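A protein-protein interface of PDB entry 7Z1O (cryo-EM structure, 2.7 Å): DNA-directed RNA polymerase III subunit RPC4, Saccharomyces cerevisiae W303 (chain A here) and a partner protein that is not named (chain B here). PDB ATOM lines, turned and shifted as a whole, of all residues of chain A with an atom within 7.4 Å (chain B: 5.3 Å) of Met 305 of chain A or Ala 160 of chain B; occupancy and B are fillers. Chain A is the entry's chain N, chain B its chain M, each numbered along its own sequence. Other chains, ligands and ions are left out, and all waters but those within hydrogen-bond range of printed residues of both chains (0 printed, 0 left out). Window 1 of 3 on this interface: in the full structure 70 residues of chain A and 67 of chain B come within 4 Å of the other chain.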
ATOM      1  N   HIS A 289       7.793   3.780 -20.688  1.00  0.00           N
ATOM      2  CA  HIS A 289       8.231   2.437 -20.318  1.00  0.00           C
ATOM      3  C   HIS A 289       9.552   2.074 -20.987  1.00  0.00           C
ATOM      4  O   HIS A 289      10.401   1.419 -20.375  1.00  0.00           O
ATOM      5  CB  HIS A 289       7.153   1.413 -20.670  1.00  0.00           C
ATOM      6  CG  HIS A 289       5.952   1.474 -19.780  1.00  0.00           C
ATOM      7  ND1 HIS A 289       4.931   0.551 -19.845  1.00  0.00           N
ATOM      8  CD2 HIS A 289       5.609   2.346 -18.804  1.00  0.00           C
ATOM      9  CE1 HIS A 289       4.010   0.852 -18.946  1.00  0.00           C
ATOM     10  NE2 HIS A 289       4.397   1.938 -18.301  1.00  0.00           N
ATOM     11  N   ILE A 290       9.741   2.486 -22.243  1.00  0.00           N
ATOM     12  CA  ILE A 290      10.991   2.214 -22.948  1.00  0.00           C
ATOM     13  C   ILE A 290      12.149   2.945 -22.283  1.00  0.00           C
ATOM     14  O   ILE A 290      13.229   2.373 -22.088  1.00  0.00           O
ATOM     15  CB  ILE A 290      10.859   2.590 -24.437  1.00  0.00           C
ATOM     16  CG1 ILE A 290      10.039   1.539 -25.182  1.00  0.00           C
ATOM     17  CG2 ILE A 290      12.223   2.746 -25.090  1.00  0.00           C
ATOM     18  CD1 ILE A 290       9.430   2.043 -26.471  1.00  0.00           C
ATOM     19  N   LYS A 293      12.886   1.155 -18.974  1.00  0.00           N
ATOM     20  CA  LYS A 293      13.527  -0.138 -19.189  1.00  0.00           C
ATOM     21  C   LYS A 293      14.967   0.027 -19.653  1.00  0.00           C
ATOM     22  O   LYS A 293      15.842  -0.759 -19.272  1.00  0.00           O
ATOM     23  CB  LYS A 293      12.725  -0.956 -20.199  1.00  0.00           C
ATOM     24  CG  LYS A 293      13.186  -2.394 -20.347  1.00  0.00           C
ATOM     25  CD  LYS A 293      12.355  -3.135 -21.379  1.00  0.00           C
ATOM     26  CE  LYS A 293      10.965  -3.441 -20.848  1.00  0.00           C
ATOM     27  NZ  LYS A 293      10.172  -4.260 -21.803  1.00  0.00           N
ATOM     28  N   LEU A 294      15.234   1.040 -20.481  1.00  0.00           N
ATOM     29  CA  LEU A 294      16.604   1.318 -20.897  1.00  0.00           C
ATOM     30  C   LEU A 294      17.457   1.755 -19.714  1.00  0.00           C
ATOM     31  O   LEU A 294      18.642   1.409 -19.634  1.00  0.00           O
ATOM     32  CB  LEU A 294      16.618   2.385 -21.991  1.00  0.00           C
ATOM     33  CG  LEU A 294      16.490   1.892 -23.431  1.00  0.00           C
ATOM     34  CD1 LEU A 294      16.291   3.061 -24.380  1.00  0.00           C
ATOM     35  CD2 LEU A 294      17.710   1.081 -23.827  1.00  0.00           C
ATOM     36  N   MET A 297      18.333  -1.422 -17.297  1.00  0.00           N
ATOM     37  CA  MET A 297      19.224  -2.468 -17.785  1.00  0.00           C
ATOM     38  C   MET A 297      20.637  -1.953 -18.033  1.00  0.00           C
ATOM     39  O   MET A 297      21.403  -2.577 -18.776  1.00  0.00           O
ATOM     40  CB  MET A 297      18.656  -3.116 -19.050  1.00  0.00           C
ATOM     41  CG  MET A 297      18.556  -2.197 -20.253  1.00  0.00           C
ATOM     42  SD  MET A 297      17.893  -3.051 -21.696  1.00  0.00           S
ATOM     43  CE  MET A 297      19.277  -4.098 -22.136  1.00  0.00           C
ATOM     44  N   ARG A 303      21.463  -9.398 -19.850  1.00  0.00           N
ATOM     45  CA  ARG A 303      20.260  -8.637 -20.155  1.00  0.00           C
ATOM     46  C   ARG A 303      20.281  -8.258 -21.627  1.00  0.00           C
ATOM     47  O   ARG A 303      21.259  -7.673 -22.106  1.00  0.00           O
ATOM     48  CB  ARG A 303      20.171  -7.373 -19.296  1.00  0.00           C
ATOM     49  CG  ARG A 303      19.971  -7.624 -17.813  1.00  0.00           C
ATOM     50  CD  ARG A 303      18.541  -7.980 -17.456  1.00  0.00           C
ATOM     51  NE  ARG A 303      18.521  -9.070 -16.488  1.00  0.00           N
ATOM     52  CZ  ARG A 303      17.424  -9.611 -15.979  1.00  0.00           C
ATOM     53  NH1 ARG A 303      16.218  -9.204 -16.343  1.00  0.00           N
ATOM     54  NH2 ARG A 303      17.540 -10.584 -15.080  1.00  0.00           N
ATOM     55  N   PHE A 304      19.209  -8.583 -22.342  1.00  0.00           N
ATOM     56  CA  PHE A 304      19.100  -8.276 -23.758  1.00  0.00           C
ATOM     57  C   PHE A 304      17.716  -7.722 -24.063  1.00  0.00           C
ATOM     58  O   PHE A 304      16.744  -7.987 -23.351  1.00  0.00           O
ATOM     59  CB  PHE A 304      19.379  -9.509 -24.627  1.00  0.00           C
ATOM     60  CG  PHE A 304      20.822  -9.667 -25.007  1.00  0.00           C
ATOM     61  CD1 PHE A 304      21.384  -8.870 -25.989  1.00  0.00           C
ATOM     62  CD2 PHE A 304      21.617 -10.612 -24.384  1.00  0.00           C
ATOM     63  CE1 PHE A 304      22.712  -9.012 -26.341  1.00  0.00           C
ATOM     64  CE2 PHE A 304      22.944 -10.760 -24.733  1.00  0.00           C
ATOM     65  CZ  PHE A 304      23.492  -9.959 -25.712  1.00  0.00           C
ATOM     66  N   MET A 305      17.644  -6.940 -25.137  1.00  0.00           N
ATOM     67  CA  MET A 305      16.394  -6.356 -25.604  1.00  0.00           C
ATOM     68  C   MET A 305      16.451  -6.264 -27.119  1.00  0.00           C
ATOM     69  O   MET A 305      17.453  -5.803 -27.673  1.00  0.00           O
ATOM     70  CB  MET A 305      16.162  -4.978 -24.975  1.00  0.00           C
ATOM     71  CG  MET A 305      14.856  -4.319 -25.365  1.00  0.00           C
ATOM     72  SD  MET A 305      14.643  -2.719 -24.563  1.00  0.00           S
ATOM     73  CE  MET A 305      15.848  -1.735 -25.447  1.00  0.00           C
ATOM     74  N   VAL A 306      15.387  -6.699 -27.785  1.00  0.00           N
ATOM     75  CA  VAL A 306      15.392  -6.852 -29.235  1.00  0.00           C
ATOM     76  C   VAL A 306      14.914  -5.567 -29.896  1.00  0.00           C
ATOM     77  O   VAL A 306      13.789  -5.108 -29.657  1.00  0.00           O
ATOM     78  CB  VAL A 306      14.523  -8.044 -29.667  1.00  0.00           C
ATOM     79  CG1 VAL A 306      14.534  -8.179 -31.178  1.00  0.00           C
ATOM     80  CG2 VAL A 306      15.030  -9.318 -29.034  1.00  0.00           C
ATOM     81  N   PHE A 307      15.763  -5.002 -30.749  1.00  0.00           N
ATOM     82  CA  PHE A 307      15.405  -3.898 -31.627  1.00  0.00           C
ATOM     83  C   PHE A 307      14.855  -4.469 -32.924  1.00  0.00           C
ATOM     84  O   PHE A 307      15.406  -5.436 -33.461  1.00  0.00           O
ATOM     85  CB  PHE A 307      16.617  -3.020 -31.948  1.00  0.00           C
ATOM     86  CG  PHE A 307      16.926  -1.977 -30.914  1.00  0.00           C
ATOM     87  CD1 PHE A 307      17.118  -2.321 -29.589  1.00  0.00           C
ATOM     88  CD2 PHE A 307      17.067  -0.650 -31.283  1.00  0.00           C
ATOM     89  CE1 PHE A 307      17.427  -1.357 -28.649  1.00  0.00           C
ATOM     90  CE2 PHE A 307      17.371   0.317 -30.346  1.00  0.00           C
ATOM     91  CZ  PHE A 307      17.557  -0.038 -29.030  1.00  0.00           C
ATOM     92  N   GLN A 308      13.778  -3.878 -33.425  1.00  0.00           N
ATOM     93  CA  GLN A 308      13.323  -4.132 -34.784  1.00  0.00           C
ATOM     94  C   GLN A 308      13.553  -2.864 -35.592  1.00  0.00           C
ATOM     95  O   GLN A 308      12.743  -1.932 -35.538  1.00  0.00           O
ATOM     96  CB  GLN A 308      11.854  -4.553 -34.832  1.00  0.00           C
ATOM     97  CG  GLN A 308      11.338  -4.747 -36.252  1.00  0.00           C
ATOM     98  CD  GLN A 308       9.962  -5.369 -36.304  1.00  0.00           C
ATOM     99  OE1 GLN A 308       9.726  -6.429 -35.726  1.00  0.00           O
ATOM    100  NE2 GLN A 308       9.045  -4.717 -37.006  1.00  0.00           N
ATOM    101  N   ILE A 363      19.464   7.759 -29.583  1.00  0.00           N
ATOM    102  CA  ILE A 363      18.114   7.743 -29.032  1.00  0.00           C
ATOM    103  C   ILE A 363      17.960   8.994 -28.180  1.00  0.00           C
ATOM    104  O   ILE A 363      18.676   9.169 -27.186  1.00  0.00           O
ATOM    105  CB  ILE A 363      17.852   6.475 -28.206  1.00  0.00           C
ATOM    106  CG1 ILE A 363      17.948   5.231 -29.090  1.00  0.00           C
ATOM    107  CG2 ILE A 363      16.491   6.547 -27.538  1.00  0.00           C
ATOM    108  CD1 ILE A 363      17.926   3.935 -28.315  1.00  0.00           C
ATOM    109  N   ILE A 382       9.499   5.367 -32.164  1.00  0.00           N
ATOM    110  CA  ILE A 382       9.863   4.169 -31.415  1.00  0.00           C
ATOM    111  C   ILE A 382       8.641   3.691 -30.640  1.00  0.00           C
ATOM    112  O   ILE A 382       7.910   4.495 -30.053  1.00  0.00           O
ATOM    113  CB  ILE A 382      11.066   4.444 -30.486  1.00  0.00           C
ATOM    114  CG1 ILE A 382      11.373   3.243 -29.592  1.00  0.00           C
ATOM    115  CG2 ILE A 382      10.842   5.696 -29.662  1.00  0.00           C
ATOM    116  CD1 ILE A 382      12.711   3.346 -28.903  1.00  0.00           C
ATOM    117  N   VAL A 394      19.073 -15.435 -25.689  1.00  0.00           N
ATOM    118  CA  VAL A 394      20.014 -15.165 -26.770  1.00  0.00           C
ATOM    119  C   VAL A 394      21.108 -16.223 -26.744  1.00  0.00           C
ATOM    120  O   VAL A 394      21.727 -16.466 -25.701  1.00  0.00           O
ATOM    121  CB  VAL A 394      20.606 -13.752 -26.637  1.00  0.00           C
ATOM    122  CG1 VAL A 394      21.721 -13.545 -27.638  1.00  0.00           C
ATOM    123  CG2 VAL A 394      19.522 -12.707 -26.826  1.00  0.00           C
ATOM    124  N   ARG A 411      18.881 -13.465 -21.383  1.00  0.00           N
ATOM    125  CA  ARG A 411      17.505 -13.563 -21.838  1.00  0.00           C
ATOM    126  C   ARG A 411      17.015 -12.202 -22.311  1.00  0.00           C
ATOM    127  O   ARG A 411      17.515 -11.153 -21.895  1.00  0.00           O
ATOM    128  CB  ARG A 411      16.576 -14.109 -20.744  1.00  0.00           C
ATOM    129  CG  ARG A 411      16.274 -13.172 -19.594  1.00  0.00           C
ATOM    130  CD  ARG A 411      15.342 -13.871 -18.617  1.00  0.00           C
ATOM    131  NE  ARG A 411      14.875 -13.004 -17.543  1.00  0.00           N
ATOM    132  CZ  ARG A 411      15.523 -12.797 -16.405  1.00  0.00           C
ATOM    133  NH1 ARG A 411      16.692 -13.368 -16.162  1.00  0.00           N
ATOM    134  NH2 ARG A 411      14.979 -12.005 -15.486  1.00  0.00           N
ATOM    135  N   VAL A 412      16.022 -12.235 -23.195  1.00  0.00           N
ATOM    136  CA  VAL A 412      15.464 -11.038 -23.811  1.00  0.00           C
ATOM    137  C   VAL A 412      14.392 -10.479 -22.888  1.00  0.00           C
ATOM    138  O   VAL A 412      13.450 -11.190 -22.514  1.00  0.00           O
ATOM    139  CB  VAL A 412      14.889 -11.343 -25.204  1.00  0.00           C
ATOM    140  CG1 VAL A 412      13.943 -10.238 -25.649  1.00  0.00           C
ATOM    141  CG2 VAL A 412      16.011 -11.533 -26.207  1.00  0.00           C
ATOM    142  N   ASP A 413      14.533  -9.211 -22.518  1.00  0.00           N
ATOM    143  CA  ASP A 413      13.562  -8.512 -21.683  1.00  0.00           C
ATOM    144  C   ASP A 413      12.885  -7.448 -22.542  1.00  0.00           C
ATOM    145  O   ASP A 413      13.318  -6.293 -22.572  1.00  0.00           O
ATOM    146  CB  ASP A 413      14.233  -7.902 -20.457  1.00  0.00           C
ATOM    147  CG  ASP A 413      13.269  -7.107 -19.597  1.00  0.00           C
ATOM    148  OD1 ASP A 413      12.164  -7.615 -19.317  1.00  0.00           O
ATOM    149  OD2 ASP A 413      13.617  -5.975 -19.203  1.00  0.00           O
ATOM    150  N   GLY A 414      11.831  -7.844 -23.242  1.00  0.00           N
ATOM    151  CA  GLY A 414      11.041  -6.920 -24.027  1.00  0.00           C
ATOM    152  C   GLY A 414      11.599  -6.688 -25.422  1.00  0.00           C
ATOM    153  O   GLY A 414      12.720  -7.071 -25.755  1.00  0.00           O
ATOM    154  N   LYS A 415      10.780  -6.037 -26.244  1.00  0.00           N
ATOM    155  CA  LYS A 415      11.111  -5.683 -27.615  1.00  0.00           C
ATOM    156  C   LYS A 415      10.768  -4.219 -27.831  1.00  0.00           C
ATOM    157  O   LYS A 415       9.850  -3.699 -27.193  1.00  0.00           O
ATOM    158  CB  LYS A 415      10.333  -6.553 -28.613  1.00  0.00           C
ATOM    159  CG  LYS A 415      10.802  -6.456 -30.052  1.00  0.00           C
ATOM    160  CD  LYS A 415      10.467  -7.717 -30.827  1.00  0.00           C
ATOM    161  CE  LYS A 415      10.934  -7.615 -32.265  1.00  0.00           C
ATOM    162  NZ  LYS A 415       9.860  -7.110 -33.158  1.00  0.00           N
ATOM    163  N   ILE A 416      11.517  -3.543 -28.702  1.00  0.00           N
ATOM    164  CA  ILE A 416      11.151  -2.207 -29.161  1.00  0.00           C
ATOM    165  C   ILE A 416      11.318  -2.152 -30.674  1.00  0.00           C
ATOM    166  O   ILE A 416      12.190  -2.824 -31.235  1.00  0.00           O
ATOM    167  CB  ILE A 416      11.966  -1.090 -28.475  1.00  0.00           C
ATOM    168  CG1 ILE A 416      13.448  -1.180 -28.802  1.00  0.00           C
ATOM    169  CG2 ILE A 416      11.775  -1.099 -26.965  1.00  0.00           C
ATOM    170  CD1 ILE A 416      14.186   0.031 -28.328  1.00  0.00           C
ATOM    171  N   LEU B  85      24.389 -14.837 -34.219  1.00  0.00           N
ATOM    172  CA  LEU B  85      23.598 -14.829 -32.997  1.00  0.00           C
ATOM    173  C   LEU B  85      22.212 -15.403 -33.262  1.00  0.00           C
ATOM    174  O   LEU B  85      21.536 -14.996 -34.213  1.00  0.00           O
ATOM    175  CB  LEU B  85      23.492 -13.405 -32.455  1.00  0.00           C
ATOM    176  CG  LEU B  85      23.309 -13.244 -30.951  1.00  0.00           C
ATOM    177  CD1 LEU B  85      24.459 -13.907 -30.221  1.00  0.00           C
ATOM    178  CD2 LEU B  85      23.220 -11.775 -30.584  1.00  0.00           C
ATOM    179  N   GLN B 158      16.363  -7.491 -37.195  1.00  0.00           N
ATOM    180  CA  GLN B 158      16.315  -7.792 -35.772  1.00  0.00           C
ATOM    181  C   GLN B 158      17.710  -7.678 -35.175  1.00  0.00           C
ATOM    182  O   GLN B 158      18.671  -8.235 -35.717  1.00  0.00           O
ATOM    183  CB  GLN B 158      15.747  -9.191 -35.531  1.00  0.00           C
ATOM    184  CG  GLN B 158      14.406  -9.424 -36.192  1.00  0.00           C
ATOM    185  CD  GLN B 158      13.247  -9.090 -35.279  1.00  0.00           C
ATOM    186  OE1 GLN B 158      13.307  -9.325 -34.073  1.00  0.00           O
ATOM    187  NE2 GLN B 158      12.188  -8.529 -35.849  1.00  0.00           N
ATOM    188  N   TYR B 159      17.818  -6.955 -34.063  1.00  0.00           N
ATOM    189  CA  TYR B 159      19.086  -6.738 -33.381  1.00  0.00           C
ATOM    190  C   TYR B 159      18.897  -6.950 -31.888  1.00  0.00           C
ATOM    191  O   TYR B 159      17.982  -6.377 -31.289  1.00  0.00           O
ATOM    192  CB  TYR B 159      19.622  -5.326 -33.644  1.00  0.00           C
ATOM    193  CG  TYR B 159      19.967  -5.037 -35.087  1.00  0.00           C
ATOM    194  CD1 TYR B 159      18.998  -4.606 -35.981  1.00  0.00           C
ATOM    195  CD2 TYR B 159      21.268  -5.175 -35.551  1.00  0.00           C
ATOM    196  CE1 TYR B 159      19.310  -4.337 -37.296  1.00  0.00           C
ATOM    197  CE2 TYR B 159      21.589  -4.906 -36.866  1.00  0.00           C
ATOM    198  CZ  TYR B 159      20.606  -4.487 -37.734  1.00  0.00           C
ATOM    199  OH  TYR B 159      20.920  -4.217 -39.045  1.00  0.00           O
ATOM    200  N   ALA B 160      19.763  -7.765 -31.291  1.00  0.00           N
ATOM    201  CA  ALA B 160      19.796  -7.936 -29.846  1.00  0.00           C
ATOM    202  C   ALA B 160      20.690  -6.861 -29.246  1.00  0.00           C
ATOM    203  O   ALA B 160      21.830  -6.681 -29.681  1.00  0.00           O
ATOM    204  CB  ALA B 160      20.306  -9.327 -29.472  1.00  0.00           C
ATOM    205  N   ALA B 161      20.175  -6.146 -28.252  1.00  0.00           N
ATOM    206  CA  ALA B 161      20.840  -4.965 -27.726  1.00  0.00           C
ATOM    207  C   ALA B 161      21.154  -5.126 -26.249  1.00  0.00           C
ATOM    208  O   ALA B 161      20.382  -5.730 -25.498  1.00  0.00           O
ATOM    209  CB  ALA B 161      19.983  -3.718 -27.917  1.00  0.00           C
ATOM    210  N   PHE B 162      22.292  -4.571 -25.840  1.00  0.00           N
ATOM    211  CA  PHE B 162      22.606  -4.422 -24.427  1.00  0.00           C
ATOM    212  C   PHE B 162      23.063  -2.989 -24.184  1.00  0.00           C
ATOM    213  O   PHE B 162      23.246  -2.206 -25.122  1.00  0.00           O
ATOM    214  CB  PHE B 162      23.642  -5.454 -23.956  1.00  0.00           C
ATOM    215  CG  PHE B 162      24.983  -5.340 -24.623  1.00  0.00           C
ATOM    216  CD1 PHE B 162      25.980  -4.551 -24.073  1.00  0.00           C
ATOM    217  CD2 PHE B 162      25.258  -6.043 -25.781  1.00  0.00           C
ATOM    218  CE1 PHE B 162      27.215  -4.450 -24.675  1.00  0.00           C
ATOM    219  CE2 PHE B 162      26.493  -5.947 -26.387  1.00  0.00           C
ATOM    220  CZ  PHE B 162      27.472  -5.151 -25.831  1.00  0.00           C
ATOM    221  N   TYR B 169      24.295  -0.973 -27.519  1.00  0.00           N
ATOM    222  CA  TYR B 169      25.037  -1.749 -28.501  1.00  0.00           C
ATOM    223  C   TYR B 169      24.122  -2.809 -29.098  1.00  0.00           C
ATOM    224  O   TYR B 169      23.424  -3.519 -28.362  1.00  0.00           O
ATOM    225  CB  TYR B 169      26.264  -2.412 -27.870  1.00  0.00           C
ATOM    226  CG  TYR B 169      27.338  -1.454 -27.397  1.00  0.00           C
ATOM    227  CD1 TYR B 169      27.190  -0.736 -26.219  1.00  0.00           C
ATOM    228  CD2 TYR B 169      28.504  -1.279 -28.126  1.00  0.00           C
ATOM    229  CE1 TYR B 169      28.169   0.134 -25.783  1.00  0.00           C
ATOM    230  CE2 TYR B 169      29.489  -0.411 -27.698  1.00  0.00           C
ATOM    231  CZ  TYR B 169      29.317   0.293 -26.527  1.00  0.00           C
ATOM    232  OH  TYR B 169      30.296   1.159 -26.098  1.00  0.00           O
ATOM    233  N   LEU B 170      24.143  -2.917 -30.424  1.00  0.00           N
ATOM    234  CA  LEU B 170      23.312  -3.839 -31.182  1.00  0.00           C
ATOM    235  C   LEU B 170      24.174  -4.906 -31.841  1.00  0.00           C
ATOM    236  O   LEU B 170      25.265  -4.624 -32.345  1.00  0.00           O
ATOM    237  CB  LEU B 170      22.524  -3.100 -32.268  1.00  0.00           C
ATOM    238  CG  LEU B 170      21.592  -1.959 -31.873  1.00  0.00           C
ATOM    239  CD1 LEU B 170      21.287  -1.096 -33.081  1.00  0.00           C
ATOM    240  CD2 LEU B 170      20.317  -2.516 -31.309  1.00  0.00           C
ATOM    241  N   VAL B 171      23.674  -6.137 -31.833  1.00  0.00           N
ATOM    242  CA  VAL B 171      24.288  -7.242 -32.563  1.00  0.00           C
ATOM    243  C   VAL B 171      23.206  -7.864 -33.437  1.00  0.00           C
ATOM    244  O   VAL B 171      22.111  -8.159 -32.936  1.00  0.00           O
ATOM    245  CB  VAL B 171      24.910  -8.279 -31.614  1.00  0.00           C
ATOM    246  CG1 VAL B 171      25.602  -9.375 -32.407  1.00  0.00           C
ATOM    247  CG2 VAL B 171      25.889  -7.616 -30.660  1.00  0.00           C
ATOM    248  N   PRO B 172      23.448  -8.052 -34.734  1.00  0.00           N
ATOM    249  CA  PRO B 172      22.419  -8.644 -35.599  1.00  0.00           C
ATOM    250  C   PRO B 172      22.063 -10.061 -35.177  1.00  0.00           C
ATOM    251  O   PRO B 172      22.925 -10.847 -34.776  1.00  0.00           O
ATOM    252  CB  PRO B 172      23.068  -8.619 -36.987  1.00  0.00           C
ATOM    253  CG  PRO B 172      24.091  -7.543 -36.908  1.00  0.00           C
ATOM    254  CD  PRO B 172      24.610  -7.578 -35.503  1.00  0.00           C
ATOM    255  N   ILE B 173      20.778 -10.380 -35.273  1.00  0.00           N
ATOM    256  CA  ILE B 173      20.261 -11.703 -34.947  1.00  0.00           C
ATOM    257  C   ILE B 173      20.078 -12.465 -36.249  1.00  0.00           C
ATOM    258  O   ILE B 173      19.346 -12.020 -37.141  1.00  0.00           O
ATOM    259  CB  ILE B 173      18.943 -11.616 -34.164  1.00  0.00           C
ATOM    260  CG1 ILE B 173      19.165 -10.923 -32.821  1.00  0.00           C
ATOM    261  CG2 ILE B 173      18.356 -12.999 -33.959  1.00  0.00           C
ATOM    262  CD1 ILE B 173      17.886 -10.565 -32.104  1.00  0.00           C
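OE1 of Gln 308 of chain A is in hydrogen-bond range of NZ of Lys 415 of chain A (2.7 Å).
N of Ile 173 of chain B lies within hydrogen-bond range of O of Gln 158 of chain B, 3.0 Å away.
The backbone carbonyl oxygen of Phe 162 of chain B is in hydrogen-bond range of the backbone NH of Tyr 169 of chain B, at 2.9 Å.
The backbone carbonyl oxygen of Gly 414 of chain A sits at hydrogen-bond distance from the backbone NH of Val 306 of chain A (3.4 Å).
The backbone carbonyl oxygen of Ala 160 of chain B sits at hydrogen-bond distance from the backbone NH of Val 171 of chain B, 2.9 Å away.
The backbone carbonyl oxygen (O) of Val 306 of chain A sits at hydrogen-bond distance from the backbone NH (N) of Ile 416 of chain A (2.9 Å).
Of the printed residues of chain B, Met 297 of chain A touches Ala 161.
Printed residues of chain A within 4 Å of Leu 170 of chain B: Phe 307 (3.5 Å).
Of the printed residues of chain B, Gln 308 of chain A touches Gln 158.
Printed residues of chain A within 4 Å of Leu 85 of chain B: Val 394 (3.7 Å).
Of the printed residues of chain B, Arg 303 of chain A touches Phe 162.
Pro 172 of chain B touches none of the printed residues of chain A.
The nearest residue of chain A that does not touch Ala 160 of chain B is Val 394 of chain A (4.4 Å).
Among the printed residues, pairs that only touch across the chains: Met 297 of chain A with Ala 161 of chain B (3.9 Å), Arg 303 of chain A with Phe 162 of chain B (3.7 Å), Phe 304 of chain A with Ala 160 of chain B (3.7 Å), Phe 304 of chain A with Ala 161 of chain B (3.3 Å), Phe 304 of chain A with Phe 162 of chain B (3.95 Å), Met 305 of chain A with Tyr 159 of chain B (3.7 Å), Met 305 of chain A with Ala 160 of chain B (3.8 Å), Val 306 of chain A with Gln 158 of chain B (3.3 Å), Val 306 of chain A with Tyr 159 of chain B (3.3 Å), Phe 307 of chain A with Gln 158 of chain B (3.4 Å), Phe 307 of chain A with Ala 161 of chain B (3.6 Å), Phe 307 of chain A with Leu 170 of chain B (3.5 Å), Val 394 of chain A with Leu 85 of chain B (3.7 Å) and Lys 415 of chain A with Gln 158 of chain B (3.4 Å).
The side-chain amide oxygen (OE1) of Gln 308 of chain A is in hydrogen-bond range of the side-chain amide nitrogen (NE2) of Gln 158 of chain B.
The backbone NH of Ala 161 of chain B lies within hydrogen-bond range of the backbone carbonyl oxygen of Met 305 of chain A (2.8 Å).
The backbone carbonyl oxygen (O) of Tyr 159 of chain B is in hydrogen-bond range of the backbone NH (N) of Phe 307 of chain A (2.7 Å).
Hydrophobic or aromatic side chains of chain B that line the printed part of chain A: Leu 85, Ala 160, Ala 161, Phe 162 and Leu 170.
Printed residues of chain A that touch a printed residue of chain B: Met 297, Arg 303, Phe 304, Met 305, Val 306, Phe 307, Gln 308, Val 394 and Lys 415.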
